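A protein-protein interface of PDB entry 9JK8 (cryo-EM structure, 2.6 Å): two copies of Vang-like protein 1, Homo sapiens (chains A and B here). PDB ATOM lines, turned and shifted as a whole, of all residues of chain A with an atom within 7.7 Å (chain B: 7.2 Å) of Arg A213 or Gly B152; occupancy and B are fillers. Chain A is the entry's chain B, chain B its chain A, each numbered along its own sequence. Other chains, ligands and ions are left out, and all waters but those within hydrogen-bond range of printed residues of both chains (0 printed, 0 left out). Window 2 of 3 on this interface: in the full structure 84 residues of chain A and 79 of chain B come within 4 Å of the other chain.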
ATOM      1  N   TRP A 207      -8.640  19.321  -9.424  1.00  0.00           N
ATOM      2  CA  TRP A 207      -8.588  20.538  -8.615  1.00  0.00           C
ATOM      3  C   TRP A 207      -9.721  20.588  -7.599  1.00  0.00           C
ATOM      4  O   TRP A 207      -9.517  21.053  -6.474  1.00  0.00           O
ATOM      5  CB  TRP A 207      -8.625  21.792  -9.491  1.00  0.00           C
ATOM      6  CG  TRP A 207      -7.333  22.113 -10.175  1.00  0.00           C
ATOM      7  CD1 TRP A 207      -7.058  22.002 -11.504  1.00  0.00           C
ATOM      8  CD2 TRP A 207      -6.134  22.596  -9.557  1.00  0.00           C
ATOM      9  NE1 TRP A 207      -5.763  22.391 -11.756  1.00  0.00           N
ATOM     10  CE2 TRP A 207      -5.174  22.758 -10.575  1.00  0.00           C
ATOM     11  CE3 TRP A 207      -5.779  22.908  -8.240  1.00  0.00           C
ATOM     12  CZ2 TRP A 207      -3.883  23.218 -10.319  1.00  0.00           C
ATOM     13  CZ3 TRP A 207      -4.497  23.363  -7.988  1.00  0.00           C
ATOM     14  CH2 TRP A 207      -3.565  23.514  -9.023  1.00  0.00           C
ATOM     15  N   LEU A 208     -10.913  20.124  -7.973  1.00  0.00           N
ATOM     16  CA  LEU A 208     -12.033  20.103  -7.040  1.00  0.00           C
ATOM     17  C   LEU A 208     -11.737  19.201  -5.848  1.00  0.00           C
ATOM     18  O   LEU A 208     -11.992  19.580  -4.700  1.00  0.00           O
ATOM     19  CB  LEU A 208     -13.301  19.650  -7.764  1.00  0.00           C
ATOM     20  CG  LEU A 208     -14.601  19.602  -6.962  1.00  0.00           C
ATOM     21  CD1 LEU A 208     -14.978  20.992  -6.473  1.00  0.00           C
ATOM     22  CD2 LEU A 208     -15.721  19.006  -7.800  1.00  0.00           C
ATOM     23  N   PHE A 209     -11.191  18.011  -6.101  1.00  0.00           N
ATOM     24  CA  PHE A 209     -10.844  17.124  -4.996  1.00  0.00           C
ATOM     25  C   PHE A 209      -9.675  17.666  -4.180  1.00  0.00           C
ATOM     26  O   PHE A 209      -9.647  17.497  -2.957  1.00  0.00           O
ATOM     27  CB  PHE A 209     -10.513  15.723  -5.502  1.00  0.00           C
ATOM     28  CG  PHE A 209     -10.303  14.728  -4.399  1.00  0.00           C
ATOM     29  CD1 PHE A 209     -11.385  14.166  -3.742  1.00  0.00           C
ATOM     30  CD2 PHE A 209      -9.024  14.384  -3.989  1.00  0.00           C
ATOM     31  CE1 PHE A 209     -11.197  13.261  -2.717  1.00  0.00           C
ATOM     32  CE2 PHE A 209      -8.832  13.485  -2.961  1.00  0.00           C
ATOM     33  CZ  PHE A 209      -9.921  12.921  -2.325  1.00  0.00           C
ATOM     34  N   TYR A 210      -8.704  18.306  -4.836  1.00  0.00           N
ATOM     35  CA  TYR A 210      -7.542  18.822  -4.123  1.00  0.00           C
ATOM     36  C   TYR A 210      -7.893  20.040  -3.283  1.00  0.00           C
ATOM     37  O   TYR A 210      -7.243  20.297  -2.264  1.00  0.00           O
ATOM     38  CB  TYR A 210      -6.433  19.159  -5.122  1.00  0.00           C
ATOM     39  CG  TYR A 210      -5.126  19.576  -4.490  1.00  0.00           C
ATOM     40  CD1 TYR A 210      -4.266  18.635  -3.941  1.00  0.00           C
ATOM     41  CD2 TYR A 210      -4.744  20.911  -4.454  1.00  0.00           C
ATOM     42  CE1 TYR A 210      -3.067  19.011  -3.366  1.00  0.00           C
ATOM     43  CE2 TYR A 210      -3.547  21.297  -3.882  1.00  0.00           C
ATOM     44  CZ  TYR A 210      -2.712  20.341  -3.340  1.00  0.00           C
ATOM     45  OH  TYR A 210      -1.520  20.720  -2.768  1.00  0.00           O
ATOM     46  N   GLY A 211      -8.909  20.796  -3.684  1.00  0.00           N
ATOM     47  CA  GLY A 211      -9.329  21.954  -2.928  1.00  0.00           C
ATOM     48  C   GLY A 211     -10.319  21.617  -1.836  1.00  0.00           C
ATOM     49  O   GLY A 211     -10.221  22.142  -0.725  1.00  0.00           O
ATOM     50  N   VAL A 212     -11.274  20.734  -2.131  1.00  0.00           N
ATOM     51  CA  VAL A 212     -12.314  20.419  -1.159  1.00  0.00           C
ATOM     52  C   VAL A 212     -11.793  19.474  -0.082  1.00  0.00           C
ATOM     53  O   VAL A 212     -11.988  19.708   1.115  1.00  0.00           O
ATOM     54  CB  VAL A 212     -13.551  19.836  -1.869  1.00  0.00           C
ATOM     55  CG1 VAL A 212     -14.545  19.298  -0.850  1.00  0.00           C
ATOM     56  CG2 VAL A 212     -14.207  20.895  -2.741  1.00  0.00           C
ATOM     57  N   ARG A 213     -11.115  18.398  -0.483  1.00  0.00           N
ATOM     58  CA  ARG A 213     -10.798  17.312   0.435  1.00  0.00           C
ATOM     59  C   ARG A 213      -9.343  17.275   0.882  1.00  0.00           C
ATOM     60  O   ARG A 213      -8.997  16.441   1.725  1.00  0.00           O
ATOM     61  CB  ARG A 213     -11.169  15.966  -0.195  1.00  0.00           C
ATOM     62  CG  ARG A 213     -12.651  15.803  -0.456  1.00  0.00           C
ATOM     63  CD  ARG A 213     -13.423  15.812   0.853  1.00  0.00           C
ATOM     64  NE  ARG A 213     -13.021  14.724   1.735  1.00  0.00           N
ATOM     65  CZ  ARG A 213     -13.562  13.514   1.728  1.00  0.00           C
ATOM     66  NH1 ARG A 213     -14.536  13.197   0.892  1.00  0.00           N
ATOM     67  NH2 ARG A 213     -13.113  12.598   2.583  1.00  0.00           N
ATOM     68  N   ILE A 214      -8.480  18.143   0.356  1.00  0.00           N
ATOM     69  CA  ILE A 214      -7.074  18.180   0.735  1.00  0.00           C
ATOM     70  C   ILE A 214      -6.683  19.533   1.314  1.00  0.00           C
ATOM     71  O   ILE A 214      -6.130  19.613   2.415  1.00  0.00           O
ATOM     72  CB  ILE A 214      -6.158  17.806  -0.454  1.00  0.00           C
ATOM     73  CG1 ILE A 214      -6.360  16.338  -0.833  1.00  0.00           C
ATOM     74  CG2 ILE A 214      -4.701  18.077  -0.111  1.00  0.00           C
ATOM     75  CD1 ILE A 214      -5.691  15.937  -2.126  1.00  0.00           C
ATOM     76  N   LEU A 215      -6.965  20.615   0.586  1.00  0.00           N
ATOM     77  CA  LEU A 215      -6.597  21.933   1.087  1.00  0.00           C
ATOM     78  C   LEU A 215      -7.496  22.395   2.229  1.00  0.00           C
ATOM     79  O   LEU A 215      -7.003  22.994   3.188  1.00  0.00           O
ATOM     80  CB  LEU A 215      -6.600  22.960  -0.049  1.00  0.00           C
ATOM     81  CG  LEU A 215      -5.544  22.750  -1.137  1.00  0.00           C
ATOM     82  CD1 LEU A 215      -5.732  23.741  -2.279  1.00  0.00           C
ATOM     83  CD2 LEU A 215      -4.137  22.851  -0.553  1.00  0.00           C
ATOM     84  N   ASP A 216      -8.801  22.128   2.166  1.00  0.00           N
ATOM     85  CA  ASP A 216      -9.671  22.565   3.254  1.00  0.00           C
ATOM     86  C   ASP A 216      -9.372  21.815   4.547  1.00  0.00           C
ATOM     87  O   ASP A 216      -9.477  22.388   5.638  1.00  0.00           O
ATOM     88  CB  ASP A 216     -11.137  22.410   2.856  1.00  0.00           C
ATOM     89  CG  ASP A 216     -11.520  23.306   1.698  1.00  0.00           C
ATOM     90  OD1 ASP A 216     -10.632  24.019   1.182  1.00  0.00           O
ATOM     91  OD2 ASP A 216     -12.704  23.301   1.302  1.00  0.00           O
ATOM     92  N   SER A 217      -8.995  20.542   4.449  1.00  0.00           N
ATOM     93  CA  SER A 217      -8.722  19.750   5.642  1.00  0.00           C
ATOM     94  C   SER A 217      -7.274  19.820   6.101  1.00  0.00           C
ATOM     95  O   SER A 217      -6.997  19.465   7.254  1.00  0.00           O
ATOM     96  CB  SER A 217      -9.106  18.285   5.410  1.00  0.00           C
ATOM     97  OG  SER A 217      -8.322  17.709   4.383  1.00  0.00           O
ATOM     98  N   ARG A 218      -6.346  20.308   5.257  1.00  0.00           N
ATOM     99  CA  ARG A 218      -4.892  20.395   5.583  1.00  0.00           C
ATOM    100  C   ARG A 218      -4.431  19.023   6.076  1.00  0.00           C
ATOM    101  O   ARG A 218      -4.037  18.842   7.232  1.00  0.00           O
ATOM    102  CB  ARG A 218      -4.589  21.489   6.612  1.00  0.00           C
ATOM    103  CG  ARG A 218      -4.839  22.906   6.120  1.00  0.00           C
ATOM    104  CD  ARG A 218      -3.760  23.358   5.150  1.00  0.00           C
ATOM    105  NE  ARG A 218      -3.809  24.798   4.915  1.00  0.00           N
ATOM    106  CZ  ARG A 218      -4.415  25.369   3.879  1.00  0.00           C
ATOM    107  NH1 ARG A 218      -5.026  24.620   2.971  1.00  0.00           N
ATOM    108  NH2 ARG A 218      -4.409  26.687   3.748  1.00  0.00           N
ATOM    109  N   ASP A 219      -4.366  18.095   5.132  1.00  0.00           N
ATOM    110  CA  ASP A 219      -4.192  16.678   5.432  1.00  0.00           C
ATOM    111  C   ASP A 219      -2.756  16.336   5.834  1.00  0.00           C
ATOM    112  O   ASP A 219      -1.794  17.033   5.498  1.00  0.00           O
ATOM    113  CB  ASP A 219      -4.597  15.820   4.231  1.00  0.00           C
ATOM    114  CG  ASP A 219      -4.972  14.401   4.621  1.00  0.00           C
ATOM    115  OD1 ASP A 219      -4.072  13.539   4.683  1.00  0.00           O
ATOM    116  OD2 ASP A 219      -6.168  14.146   4.870  1.00  0.00           O
ATOM    117  N   GLU B 149     -11.271  -0.184   7.737  1.00  0.00           N
ATOM    118  CA  GLU B 149     -10.567   0.929   8.345  1.00  0.00           C
ATOM    119  C   GLU B 149     -10.909   2.219   7.601  1.00  0.00           C
ATOM    120  O   GLU B 149     -11.175   2.196   6.396  1.00  0.00           O
ATOM    121  CB  GLU B 149      -9.059   0.689   8.310  1.00  0.00           C
ATOM    122  CG  GLU B 149      -8.591  -0.465   9.184  1.00  0.00           C
ATOM    123  CD  GLU B 149      -7.092  -0.684   9.106  1.00  0.00           C
ATOM    124  OE1 GLU B 149      -6.435  -0.019   8.278  1.00  0.00           O
ATOM    125  OE2 GLU B 149      -6.571  -1.521   9.872  1.00  0.00           O
ATOM    126  N   PRO B 150     -10.921   3.359   8.295  1.00  0.00           N
ATOM    127  CA  PRO B 150     -11.286   4.622   7.633  1.00  0.00           C
ATOM    128  C   PRO B 150     -10.210   5.058   6.646  1.00  0.00           C
ATOM    129  O   PRO B 150      -9.067   5.320   7.026  1.00  0.00           O
ATOM    130  CB  PRO B 150     -11.422   5.610   8.798  1.00  0.00           C
ATOM    131  CG  PRO B 150     -10.591   5.024   9.889  1.00  0.00           C
ATOM    132  CD  PRO B 150     -10.708   3.534   9.742  1.00  0.00           C
ATOM    133  N   CYS B 151     -10.590   5.134   5.370  1.00  0.00           N
ATOM    134  CA  CYS B 151      -9.676   5.593   4.328  1.00  0.00           C
ATOM    135  C   CYS B 151      -9.606   7.116   4.290  1.00  0.00           C
ATOM    136  O   CYS B 151      -8.539   7.706   4.493  1.00  0.00           O
ATOM    137  CB  CYS B 151     -10.117   5.035   2.974  1.00  0.00           C
ATOM    138  SG  CYS B 151     -11.750   5.616   2.454  1.00  0.00           S
ATOM    139  N   GLY B 152     -10.730   7.763   4.027  1.00  0.00           N
ATOM    140  CA  GLY B 152     -10.812   9.225   4.086  1.00  0.00           C
ATOM    141  C   GLY B 152     -10.559   9.866   2.725  1.00  0.00           C
ATOM    142  O   GLY B 152     -11.391   9.768   1.824  1.00  0.00           O
ATOM    143  N   THR B 153      -9.408  10.526   2.584  1.00  0.00           N
ATOM    144  CA  THR B 153      -9.089  11.318   1.407  1.00  0.00           C
ATOM    145  C   THR B 153      -8.414  10.495   0.318  1.00  0.00           C
ATOM    146  O   THR B 153      -8.755  10.615  -0.868  1.00  0.00           O
ATOM    147  CB  THR B 153      -8.192  12.498   1.800  1.00  0.00           C
ATOM    148  OG1 THR B 153      -8.867  13.304   2.776  1.00  0.00           O
ATOM    149  CG2 THR B 153      -7.855  13.348   0.588  1.00  0.00           C
ATOM    150  N   ILE B 154      -7.455   9.651   0.700  1.00  0.00           N
ATOM    151  CA  ILE B 154      -6.678   8.924  -0.289  1.00  0.00           C
ATOM    152  C   ILE B 154      -7.564   7.988  -1.090  1.00  0.00           C
ATOM    153  O   ILE B 154      -7.473   7.933  -2.320  1.00  0.00           O
ATOM    154  CB  ILE B 154      -5.528   8.176   0.410  1.00  0.00           C
ATOM    155  CG1 ILE B 154      -4.682   9.221   1.124  1.00  0.00           C
ATOM    156  CG2 ILE B 154      -4.699   7.378  -0.586  1.00  0.00           C
ATOM    157  CD1 ILE B 154      -4.108  10.194   0.171  1.00  0.00           C
ATOM    158  N   CYS B 155      -8.465   7.274  -0.421  1.00  0.00           N
ATOM    159  CA  CYS B 155      -9.305   6.310  -1.121  1.00  0.00           C
ATOM    160  C   CYS B 155     -10.148   6.981  -2.199  1.00  0.00           C
ATOM    161  O   CYS B 155     -10.284   6.449  -3.305  1.00  0.00           O
ATOM    162  CB  CYS B 155     -10.197   5.568  -0.128  1.00  0.00           C
ATOM    163  SG  CYS B 155     -11.399   6.612   0.722  1.00  0.00           S
ATOM    164  N   GLU B 156     -10.712   8.158  -1.911  1.00  0.00           N
ATOM    165  CA  GLU B 156     -11.541   8.834  -2.907  1.00  0.00           C
ATOM    166  C   GLU B 156     -10.691   9.465  -4.007  1.00  0.00           C
ATOM    167  O   GLU B 156     -11.074   9.448  -5.189  1.00  0.00           O
ATOM    168  CB  GLU B 156     -12.420   9.882  -2.227  1.00  0.00           C
ATOM    169  CG  GLU B 156     -13.474   9.283  -1.307  1.00  0.00           C
ATOM    170  CD  GLU B 156     -14.340  10.335  -0.645  1.00  0.00           C
ATOM    171  OE1 GLU B 156     -14.050  11.538  -0.812  1.00  0.00           O
ATOM    172  OE2 GLU B 156     -15.312   9.959   0.044  1.00  0.00           O
ATOM    173  N   GLY B 157      -9.537  10.035  -3.643  1.00  0.00           N
ATOM    174  CA  GLY B 157      -8.629  10.569  -4.644  1.00  0.00           C
ATOM    175  C   GLY B 157      -8.073   9.515  -5.571  1.00  0.00           C
ATOM    176  O   GLY B 157      -7.557   9.843  -6.643  1.00  0.00           O
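Hydrophobic or aromatic side chains of chain A within 4 Å of the printed part of chain B: Phe A209 and Ile A214. Among the printed residues, 8 pairs touch across the chains. Among the printed residues, Asp or Glu carboxylates within 4 Å of a Lys or Arg side-chain nitrogen of the other chain: Arg A213 with Glu B156 (2.4 Å).
Printed residues of chain B within 4 Å of Arg A213: Gly B152 (3.4 Å), Thr B153 (3.3 Å) and Glu B156 (2.4 Å). No residue of chain A comes within 4 Å of Cys B151. Of the printed residues of chain A, Glu B156 touches Phe A209 and Arg A213. Of the printed residues of chain A, Gly B157 touches Phe A209. Of the printed residues of chain B, Phe A209 touches Thr B153, Glu B156 and Gly B157. Printed residues of chain B within 4 Å of Asp A219: Thr B153. Printed residues of chain A within 4 Å of Thr B153: Phe A209, Arg A213, Ile A214 and Asp A219. The nearest residue of chain B that does not touch Arg A213 is Cys B155 (6.5 Å). The nearest printed residue of chain A that does not touch Thr B153 is Ser A217 (4.7 Å).
O of Gly B152 lies within hydrogen-bond range of NH2 of Arg A213. O of Arg A213 lies within hydrogen-bond range of OG1 of Thr B153. The side-chain carboxylate (OE1) of Glu B156 is in salt-bridge range of the guanidinium group (NH1) of Arg A213.
CZ of Phe A209 touches O of Thr B153, 3.0 Å away. Glu B156 touches Phe A209 (CB to CE1, 3.6 Å). Phe A209 touches Gly B157 (CZ to N, 3.2 Å). Ile A214 touches Thr B153. Asp A219 touches Thr B153 (OD2 to OG1, 3.5 Å).
No position is printed for both chains. Of the 8 pairs that touch across the chains among the printed residues, none has its exchanged pair printed and touching as well.
N of Gly B152 is in hydrogen-bond range of SG of Cys B155 (3.6 Å). O of Arg A213 sits at hydrogen-bond distance from OG of Ser A217. The side-chain sulfur of Cys B155 is disulfide-bonded to the side-chain sulfur of Cys B151.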
